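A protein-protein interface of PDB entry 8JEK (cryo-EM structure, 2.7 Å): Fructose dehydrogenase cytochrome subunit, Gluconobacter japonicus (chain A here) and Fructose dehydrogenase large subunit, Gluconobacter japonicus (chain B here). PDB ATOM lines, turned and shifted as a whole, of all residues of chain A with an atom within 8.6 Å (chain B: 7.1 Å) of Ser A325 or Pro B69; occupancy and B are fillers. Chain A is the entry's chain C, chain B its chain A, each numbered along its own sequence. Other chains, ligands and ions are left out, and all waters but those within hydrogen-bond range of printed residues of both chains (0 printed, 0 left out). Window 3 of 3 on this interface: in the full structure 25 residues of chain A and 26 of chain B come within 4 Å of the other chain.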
ATOM      1  N   ALA A 320     -23.905  10.673  23.210  1.00  0.00           N
ATOM      2  CA  ALA A 320     -22.944   9.698  23.703  1.00  0.00           C
ATOM      3  C   ALA A 320     -21.678   9.641  22.863  1.00  0.00           C
ATOM      4  O   ALA A 320     -20.677   9.081  23.324  1.00  0.00           O
ATOM      5  CB  ALA A 320     -23.585   8.313  23.758  1.00  0.00           C
ATOM      6  N   ASN A 321     -21.692  10.204  21.652  1.00  0.00           N
ATOM      7  CA  ASN A 321     -20.499  10.168  20.814  1.00  0.00           C
ATOM      8  C   ASN A 321     -19.335  10.920  21.438  1.00  0.00           C
ATOM      9  O   ASN A 321     -18.178  10.613  21.133  1.00  0.00           O
ATOM     10  CB  ASN A 321     -20.804  10.742  19.432  1.00  0.00           C
ATOM     11  CG  ASN A 321     -21.941  10.028  18.744  1.00  0.00           C
ATOM     12  OD1 ASN A 321     -21.981   8.801  18.703  1.00  0.00           O
ATOM     13  ND2 ASN A 321     -22.872  10.793  18.194  1.00  0.00           N
ATOM     14  N   SER A 322     -19.611  11.899  22.300  1.00  0.00           N
ATOM     15  CA  SER A 322     -18.537  12.591  22.999  1.00  0.00           C
ATOM     16  C   SER A 322     -17.858  11.686  24.018  1.00  0.00           C
ATOM     17  O   SER A 322     -16.680  11.884  24.331  1.00  0.00           O
ATOM     18  CB  SER A 322     -19.077  13.842  23.689  1.00  0.00           C
ATOM     19  OG  SER A 322     -19.981  13.499  24.724  1.00  0.00           O
ATOM     20  N   ARG A 323     -18.577  10.697  24.541  1.00  0.00           N
ATOM     21  CA  ARG A 323     -18.046   9.827  25.579  1.00  0.00           C
ATOM     22  C   ARG A 323     -17.327   8.606  25.026  1.00  0.00           C
ATOM     23  O   ARG A 323     -16.875   7.766  25.808  1.00  0.00           O
ATOM     24  CB  ARG A 323     -19.165   9.386  26.525  1.00  0.00           C
ATOM     25  CG  ARG A 323     -19.328  10.302  27.718  1.00  0.00           C
ATOM     26  CD  ARG A 323     -20.512   9.919  28.579  1.00  0.00           C
ATOM     27  NE  ARG A 323     -21.626   9.375  27.815  1.00  0.00           N
ATOM     28  CZ  ARG A 323     -22.727  10.049  27.520  1.00  0.00           C
ATOM     29  NH1 ARG A 323     -22.877  11.315  27.870  1.00  0.00           N
ATOM     30  NH2 ARG A 323     -23.706   9.436  26.864  1.00  0.00           N
ATOM     31  N   ARG A 324     -17.222   8.477  23.708  1.00  0.00           N
ATOM     32  CA  ARG A 324     -16.345   7.464  23.145  1.00  0.00           C
ATOM     33  C   ARG A 324     -14.898   7.815  23.464  1.00  0.00           C
ATOM     34  O   ARG A 324     -14.555   8.980  23.680  1.00  0.00           O
ATOM     35  CB  ARG A 324     -16.557   7.348  21.636  1.00  0.00           C
ATOM     36  CG  ARG A 324     -17.991   7.024  21.253  1.00  0.00           C
ATOM     37  CD  ARG A 324     -18.132   6.760  19.769  1.00  0.00           C
ATOM     38  NE  ARG A 324     -17.768   7.919  18.965  1.00  0.00           N
ATOM     39  CZ  ARG A 324     -18.111   8.087  17.696  1.00  0.00           C
ATOM     40  NH1 ARG A 324     -18.834   7.187  17.050  1.00  0.00           N
ATOM     41  NH2 ARG A 324     -17.715   9.184  17.057  1.00  0.00           N
ATOM     42  N   SER A 325     -14.051   6.789  23.515  1.00  0.00           N
ATOM     43  CA  SER A 325     -12.670   6.909  23.983  1.00  0.00           C
ATOM     44  C   SER A 325     -12.595   7.340  25.444  1.00  0.00           C
ATOM     45  O   SER A 325     -11.618   7.968  25.858  1.00  0.00           O
ATOM     46  CB  SER A 325     -11.854   7.869  23.110  1.00  0.00           C
ATOM     47  OG  SER A 325     -12.050   9.212  23.514  1.00  0.00           O
ATOM     48  N   ASN A 326     -13.614   7.007  26.235  1.00  0.00           N
ATOM     49  CA  ASN A 326     -13.655   7.360  27.648  1.00  0.00           C
ATOM     50  C   ASN A 326     -13.930   6.140  28.516  1.00  0.00           C
ATOM     51  O   ASN A 326     -14.875   6.149  29.310  1.00  0.00           O
ATOM     52  CB  ASN A 326     -14.708   8.439  27.919  1.00  0.00           C
ATOM     53  CG  ASN A 326     -14.138   9.840  27.857  1.00  0.00           C
ATOM     54  OD1 ASN A 326     -14.552  10.657  27.035  1.00  0.00           O
ATOM     55  ND2 ASN A 326     -13.181  10.127  28.729  1.00  0.00           N
ATOM     56  N   SER A 327     -13.122   5.089  28.363  1.00  0.00           N
ATOM     57  CA  SER A 327     -13.265   3.848  29.122  1.00  0.00           C
ATOM     58  C   SER A 327     -13.397   4.102  30.620  1.00  0.00           C
ATOM     59  O   SER A 327     -13.007   5.167  31.105  1.00  0.00           O
ATOM     60  CB  SER A 327     -12.072   2.925  28.861  1.00  0.00           C
ATOM     61  OG  SER A 327     -10.866   3.493  29.338  1.00  0.00           O
ATOM     62  N   THR A 328     -13.984   3.142  31.341  1.00  0.00           N
ATOM     63  CA  THR A 328     -14.251   3.221  32.779  1.00  0.00           C
ATOM     64  C   THR A 328     -15.100   4.453  33.110  1.00  0.00           C
ATOM     65  O   THR A 328     -14.628   5.428  33.699  1.00  0.00           O
ATOM     66  CB  THR A 328     -12.943   3.080  33.605  1.00  0.00           C
ATOM     67  OG1 THR A 328     -13.250   2.564  34.908  1.00  0.00           O
ATOM     68  CG2 THR A 328     -12.068   4.342  33.734  1.00  0.00           C
ATOM     69  N   LYS A 331     -17.285  10.130  33.398  1.00  0.00           N
ATOM     70  CA  LYS A 331     -17.883  11.317  32.813  1.00  0.00           C
ATOM     71  C   LYS A 331     -19.311  11.074  32.351  1.00  0.00           C
ATOM     72  O   LYS A 331     -19.928  11.978  31.781  1.00  0.00           O
ATOM     73  CB  LYS A 331     -17.034  11.805  31.636  1.00  0.00           C
ATOM     74  CG  LYS A 331     -15.574  12.025  31.982  1.00  0.00           C
ATOM     75  CD  LYS A 331     -14.795  12.534  30.785  1.00  0.00           C
ATOM     76  CE  LYS A 331     -13.348  12.815  31.151  1.00  0.00           C
ATOM     77  NZ  LYS A 331     -12.612  11.573  31.509  1.00  0.00           N
ATOM     78  N   PRO B  40      -5.302   0.301  31.434  1.00  0.00           N
ATOM     79  CA  PRO B  40      -6.131   0.915  32.479  1.00  0.00           C
ATOM     80  C   PRO B  40      -7.243   0.006  32.973  1.00  0.00           C
ATOM     81  O   PRO B  40      -7.393  -1.123  32.501  1.00  0.00           O
ATOM     82  CB  PRO B  40      -6.704   2.146  31.773  1.00  0.00           C
ATOM     83  CG  PRO B  40      -6.832   1.707  30.353  1.00  0.00           C
ATOM     84  CD  PRO B  40      -5.713   0.728  30.085  1.00  0.00           C
ATOM     85  N   ARG B  42     -11.238  -0.813  33.064  1.00  0.00           N
ATOM     86  CA  ARG B  42     -12.298  -0.655  32.080  1.00  0.00           C
ATOM     87  C   ARG B  42     -13.638  -1.024  32.697  1.00  0.00           C
ATOM     88  O   ARG B  42     -13.720  -1.935  33.526  1.00  0.00           O
ATOM     89  CB  ARG B  42     -12.037  -1.518  30.843  1.00  0.00           C
ATOM     90  CG  ARG B  42     -10.602  -1.486  30.356  1.00  0.00           C
ATOM     91  CD  ARG B  42     -10.522  -1.817  28.885  1.00  0.00           C
ATOM     92  NE  ARG B  42      -9.226  -1.481  28.308  1.00  0.00           N
ATOM     93  CZ  ARG B  42      -8.956  -0.343  27.686  1.00  0.00           C
ATOM     94  NH1 ARG B  42      -9.862   0.612  27.568  1.00  0.00           N
ATOM     95  NH2 ARG B  42      -7.746  -0.159  27.165  1.00  0.00           N
ATOM     96  N   GLN B  46     -19.385   1.070  29.944  1.00  0.00           N
ATOM     97  CA  GLN B  46     -18.758   2.039  29.059  1.00  0.00           C
ATOM     98  C   GLN B  46     -18.338   1.418  27.733  1.00  0.00           C
ATOM     99  O   GLN B  46     -18.515   2.038  26.682  1.00  0.00           O
ATOM    100  CB  GLN B  46     -17.553   2.681  29.744  1.00  0.00           C
ATOM    101  CG  GLN B  46     -16.972   3.862  28.985  1.00  0.00           C
ATOM    102  CD  GLN B  46     -18.027   4.845  28.512  1.00  0.00           C
ATOM    103  OE1 GLN B  46     -18.716   5.468  29.314  1.00  0.00           O
ATOM    104  NE2 GLN B  46     -18.143   5.004  27.201  1.00  0.00           N
ATOM    105  N   ILE B  47     -17.790   0.202  27.756  1.00  0.00           N
ATOM    106  CA  ILE B  47     -17.463  -0.478  26.507  1.00  0.00           C
ATOM    107  C   ILE B  47     -18.728  -0.793  25.724  1.00  0.00           C
ATOM    108  O   ILE B  47     -18.734  -0.738  24.488  1.00  0.00           O
ATOM    109  CB  ILE B  47     -16.638  -1.751  26.780  1.00  0.00           C
ATOM    110  CG1 ILE B  47     -15.413  -1.437  27.643  1.00  0.00           C
ATOM    111  CG2 ILE B  47     -16.220  -2.405  25.478  1.00  0.00           C
ATOM    112  CD1 ILE B  47     -14.628  -0.211  27.205  1.00  0.00           C
ATOM    113  N   ASN B  50     -19.692   2.370  24.082  1.00  0.00           N
ATOM    114  CA  ASN B  50     -18.750   2.640  23.004  1.00  0.00           C
ATOM    115  C   ASN B  50     -19.012   1.782  21.775  1.00  0.00           C
ATOM    116  O   ASN B  50     -18.864   2.274  20.653  1.00  0.00           O
ATOM    117  CB  ASN B  50     -17.319   2.416  23.489  1.00  0.00           C
ATOM    118  CG  ASN B  50     -16.871   3.460  24.484  1.00  0.00           C
ATOM    119  OD1 ASN B  50     -17.616   4.380  24.812  1.00  0.00           O
ATOM    120  ND2 ASN B  50     -15.649   3.321  24.977  1.00  0.00           N
ATOM    121  N   ALA B  65     -11.906  -3.964  18.543  1.00  0.00           N
ATOM    122  CA  ALA B  65     -10.962  -3.175  19.319  1.00  0.00           C
ATOM    123  C   ALA B  65     -11.361  -1.721  19.506  1.00  0.00           C
ATOM    124  O   ALA B  65     -10.892  -1.098  20.462  1.00  0.00           O
ATOM    125  CB  ALA B  65      -9.569  -3.217  18.670  1.00  0.00           C
ATOM    126  N   THR B  66     -12.191  -1.162  18.628  1.00  0.00           N
ATOM    127  CA  THR B  66     -12.612   0.227  18.787  1.00  0.00           C
ATOM    128  C   THR B  66     -13.339   0.502  20.101  1.00  0.00           C
ATOM    129  O   THR B  66     -13.065   1.552  20.709  1.00  0.00           O
ATOM    130  CB  THR B  66     -13.471   0.646  17.587  1.00  0.00           C
ATOM    131  OG1 THR B  66     -12.699   0.532  16.387  1.00  0.00           O
ATOM    132  CG2 THR B  66     -13.939   2.079  17.737  1.00  0.00           C
ATOM    133  N   PRO B  67     -14.248  -0.349  20.593  1.00  0.00           N
ATOM    134  CA  PRO B  67     -14.903  -0.043  21.876  1.00  0.00           C
ATOM    135  C   PRO B  67     -13.944   0.067  23.047  1.00  0.00           C
ATOM    136  O   PRO B  67     -14.307   0.664  24.067  1.00  0.00           O
ATOM    137  CB  PRO B  67     -15.875  -1.213  22.058  1.00  0.00           C
ATOM    138  CG  PRO B  67     -16.165  -1.658  20.684  1.00  0.00           C
ATOM    139  CD  PRO B  67     -14.871  -1.523  19.954  1.00  0.00           C
ATOM    140  N   TYR B  68     -12.740  -0.493  22.942  1.00  0.00           N
ATOM    141  CA  TYR B  68     -11.736  -0.357  23.985  1.00  0.00           C
ATOM    142  C   TYR B  68     -10.733   0.702  23.569  1.00  0.00           C
ATOM    143  O   TYR B  68      -9.953   0.469  22.635  1.00  0.00           O
ATOM    144  CB  TYR B  68     -11.031  -1.688  24.232  1.00  0.00           C
ATOM    145  CG  TYR B  68     -11.961  -2.805  24.622  1.00  0.00           C
ATOM    146  CD1 TYR B  68     -12.571  -3.596  23.657  1.00  0.00           C
ATOM    147  CD2 TYR B  68     -12.234  -3.070  25.955  1.00  0.00           C
ATOM    148  CE1 TYR B  68     -13.423  -4.614  24.011  1.00  0.00           C
ATOM    149  CE2 TYR B  68     -13.085  -4.089  26.316  1.00  0.00           C
ATOM    150  CZ  TYR B  68     -13.676  -4.858  25.341  1.00  0.00           C
ATOM    151  OH  TYR B  68     -14.527  -5.874  25.698  1.00  0.00           O
ATOM    152  N   PRO B  69     -10.713   1.870  24.210  1.00  0.00           N
ATOM    153  CA  PRO B  69      -9.756   2.911  23.819  1.00  0.00           C
ATOM    154  C   PRO B  69      -8.326   2.476  24.109  1.00  0.00           C
ATOM    155  O   PRO B  69      -8.030   1.931  25.173  1.00  0.00           O
ATOM    156  CB  PRO B  69     -10.167   4.115  24.673  1.00  0.00           C
ATOM    157  CG  PRO B  69     -11.543   3.797  25.162  1.00  0.00           C
ATOM    158  CD  PRO B  69     -11.617   2.322  25.277  1.00  0.00           C
ATOM    159  N   SER B  70      -7.442   2.727  23.149  1.00  0.00           N
ATOM    160  CA  SER B  70      -6.037   2.370  23.272  1.00  0.00           C
ATOM    161  C   SER B  70      -5.278   3.512  23.935  1.00  0.00           C
ATOM    162  O   SER B  70      -5.332   4.654  23.471  1.00  0.00           O
ATOM    163  CB  SER B  70      -5.445   2.060  21.897  1.00  0.00           C
ATOM    164  OG  SER B  70      -4.097   1.650  21.997  1.00  0.00           O
ATOM    165  N   VAL B  71      -4.578   3.200  25.022  1.00  0.00           N
ATOM    166  CA  VAL B  71      -3.823   4.203  25.769  1.00  0.00           C
ATOM    167  C   VAL B  71      -2.425   4.321  25.171  1.00  0.00           C
ATOM    168  O   VAL B  71      -1.839   3.310  24.759  1.00  0.00           O
ATOM    169  CB  VAL B  71      -3.777   3.862  27.267  1.00  0.00           C
ATOM    170  CG1 VAL B  71      -5.175   3.900  27.853  1.00  0.00           C
ATOM    171  CG2 VAL B  71      -3.150   2.502  27.494  1.00  0.00           C
ATOM    172  N   ALA B  74       0.432   2.074  26.857  1.00  0.00           N
ATOM    173  CA  ALA B  74       0.256   0.637  26.660  1.00  0.00           C
ATOM    174  C   ALA B  74      -0.738   0.422  25.528  1.00  0.00           C
ATOM    175  O   ALA B  74      -1.888   0.027  25.762  1.00  0.00           O
ATOM    176  CB  ALA B  74      -0.215  -0.045  27.943  1.00  0.00           C
ATOM    177  N   HIS B  76      -2.712  -1.210  22.336  1.00  0.00           N
ATOM    178  CA  HIS B  76      -3.054  -2.521  21.810  1.00  0.00           C
ATOM    179  C   HIS B  76      -3.463  -2.377  20.348  1.00  0.00           C
ATOM    180  O   HIS B  76      -3.553  -1.273  19.809  1.00  0.00           O
ATOM    181  CB  HIS B  76      -4.145  -3.196  22.648  1.00  0.00           C
ATOM    182  CG  HIS B  76      -5.390  -2.382  22.819  1.00  0.00           C
ATOM    183  ND1 HIS B  76      -6.285  -2.160  21.794  1.00  0.00           N
ATOM    184  CD2 HIS B  76      -5.908  -1.766  23.908  1.00  0.00           C
ATOM    185  CE1 HIS B  76      -7.290  -1.428  22.240  1.00  0.00           C
ATOM    186  NE2 HIS B  76      -7.086  -1.178  23.519  1.00  0.00           N
ATOM    187  N   ILE B 101      -6.170  -6.642  23.906  1.00  0.00           N
ATOM    188  CA  ILE B 101      -6.638  -5.522  24.714  1.00  0.00           C
ATOM    189  C   ILE B 101      -5.772  -5.442  25.959  1.00  0.00           C
ATOM    190  O   ILE B 101      -5.483  -6.462  26.592  1.00  0.00           O
ATOM    191  CB  ILE B 101      -8.127  -5.656  25.099  1.00  0.00           C
ATOM    192  CG1 ILE B 101      -8.984  -5.918  23.864  1.00  0.00           C
ATOM    193  CG2 ILE B 101      -8.609  -4.411  25.821  1.00  0.00           C
ATOM    194  CD1 ILE B 101      -9.152  -4.734  22.950  1.00  0.00           C
ATOM    195  N   LYS B 102      -5.352  -4.232  26.306  1.00  0.00           N
ATOM    196  CA  LYS B 102      -4.536  -3.990  27.485  1.00  0.00           C
ATOM    197  C   LYS B 102      -5.393  -3.349  28.564  1.00  0.00           C
ATOM    198  O   LYS B 102      -6.034  -2.320  28.326  1.00  0.00           O
ATOM    199  CB  LYS B 102      -3.338  -3.100  27.151  1.00  0.00           C
ATOM    200  CG  LYS B 102      -2.461  -3.655  26.046  1.00  0.00           C
ATOM    201  CD  LYS B 102      -0.994  -3.534  26.387  1.00  0.00           C
ATOM    202  CE  LYS B 102      -0.134  -4.183  25.320  1.00  0.00           C
ATOM    203  NZ  LYS B 102       1.052  -3.354  24.986  1.00  0.00           N
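The side-chain amide nitrogen of Gln B46 sits at hydrogen-bond distance from the backbone carbonyl oxygen of Arg A323 (3.3 Å).
OD1 of Asn B50 is in hydrogen-bond range of NE2 of Gln B46 (2.5 Å).
The guanidinium group (NE) of Arg A324 sits at hydrogen-bond distance from the backbone carbonyl oxygen (O) of Asn A321, 3.5 Å away.
ND2 of Asn B50 sits at hydrogen-bond distance from O of Pro B67 (3.1 Å).
NZ of Lys A331 sits close to ND2 of Asn A326, at 3.2 Å.
O of Pro B69 lies within hydrogen-bond range of NH2 of Arg B42, at 2.9 Å.
The guanidinium group (NH2) of Arg B42 sits at hydrogen-bond distance from the backbone carbonyl oxygen (O) of Lys B102 (3.0 Å).
Arg A323 touches Asn B50 (O to OD1, 3.6 Å).
Arg A324 touches Asn B50 (CA to OD1, 3.7 Å).
Ser A325 touches Pro B69 (CA to CG, 3.5 Å).
Gln B46 touches Asn A326 (CG to O, 3.1 Å).
Pro B69 touches Asn A326.
Ser A327 touches Arg B42.
Ser A327 touches Gln B46.
Ser A327 touches Pro B69 (CB to CD, 3.7 Å).
N of Thr A328 touches CG of Gln B46, at 3.9 Å.
Asn A321 touches none of the printed residues of chain B.
Printed residues of chain B within 4 Å of Arg A323: Gln B46 (3.3 Å) and Asn B50 (3.6 Å).
Ser A325 touches just one residue of chain B: Pro B69.
Printed residues of chain B within 4 Å of Thr A328: Gln B46 (3.9 Å).
Lys A331 touches none of the printed residues of chain B.
Of the printed residues of chain A, Arg B42 touches Ser A327.
Of the printed residues of chain A, Gln B46 touches Arg A323, Asn A326, Ser A327 and Thr A328.
Of chain A, only Ser A325 (3.5 Å), Asn A326 (3.97 Å) and Ser A327 (3.7 Å) come within 4 Å of Pro B69.
The nearest residue of chain B that does not touch Ser A325 is Asn B50 (4.1 Å).
Printed residues of chain B that touch a printed residue of chain A: Arg B42, Gln B46, Asn B50 and Pro B69.
Of the 10 printed residues of chain A, 6 touch a printed residue of chain B.
Among the printed residues, no Asp or Glu carboxylate lies within 4 Å of a Lys or Arg side-chain nitrogen of the other chain.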
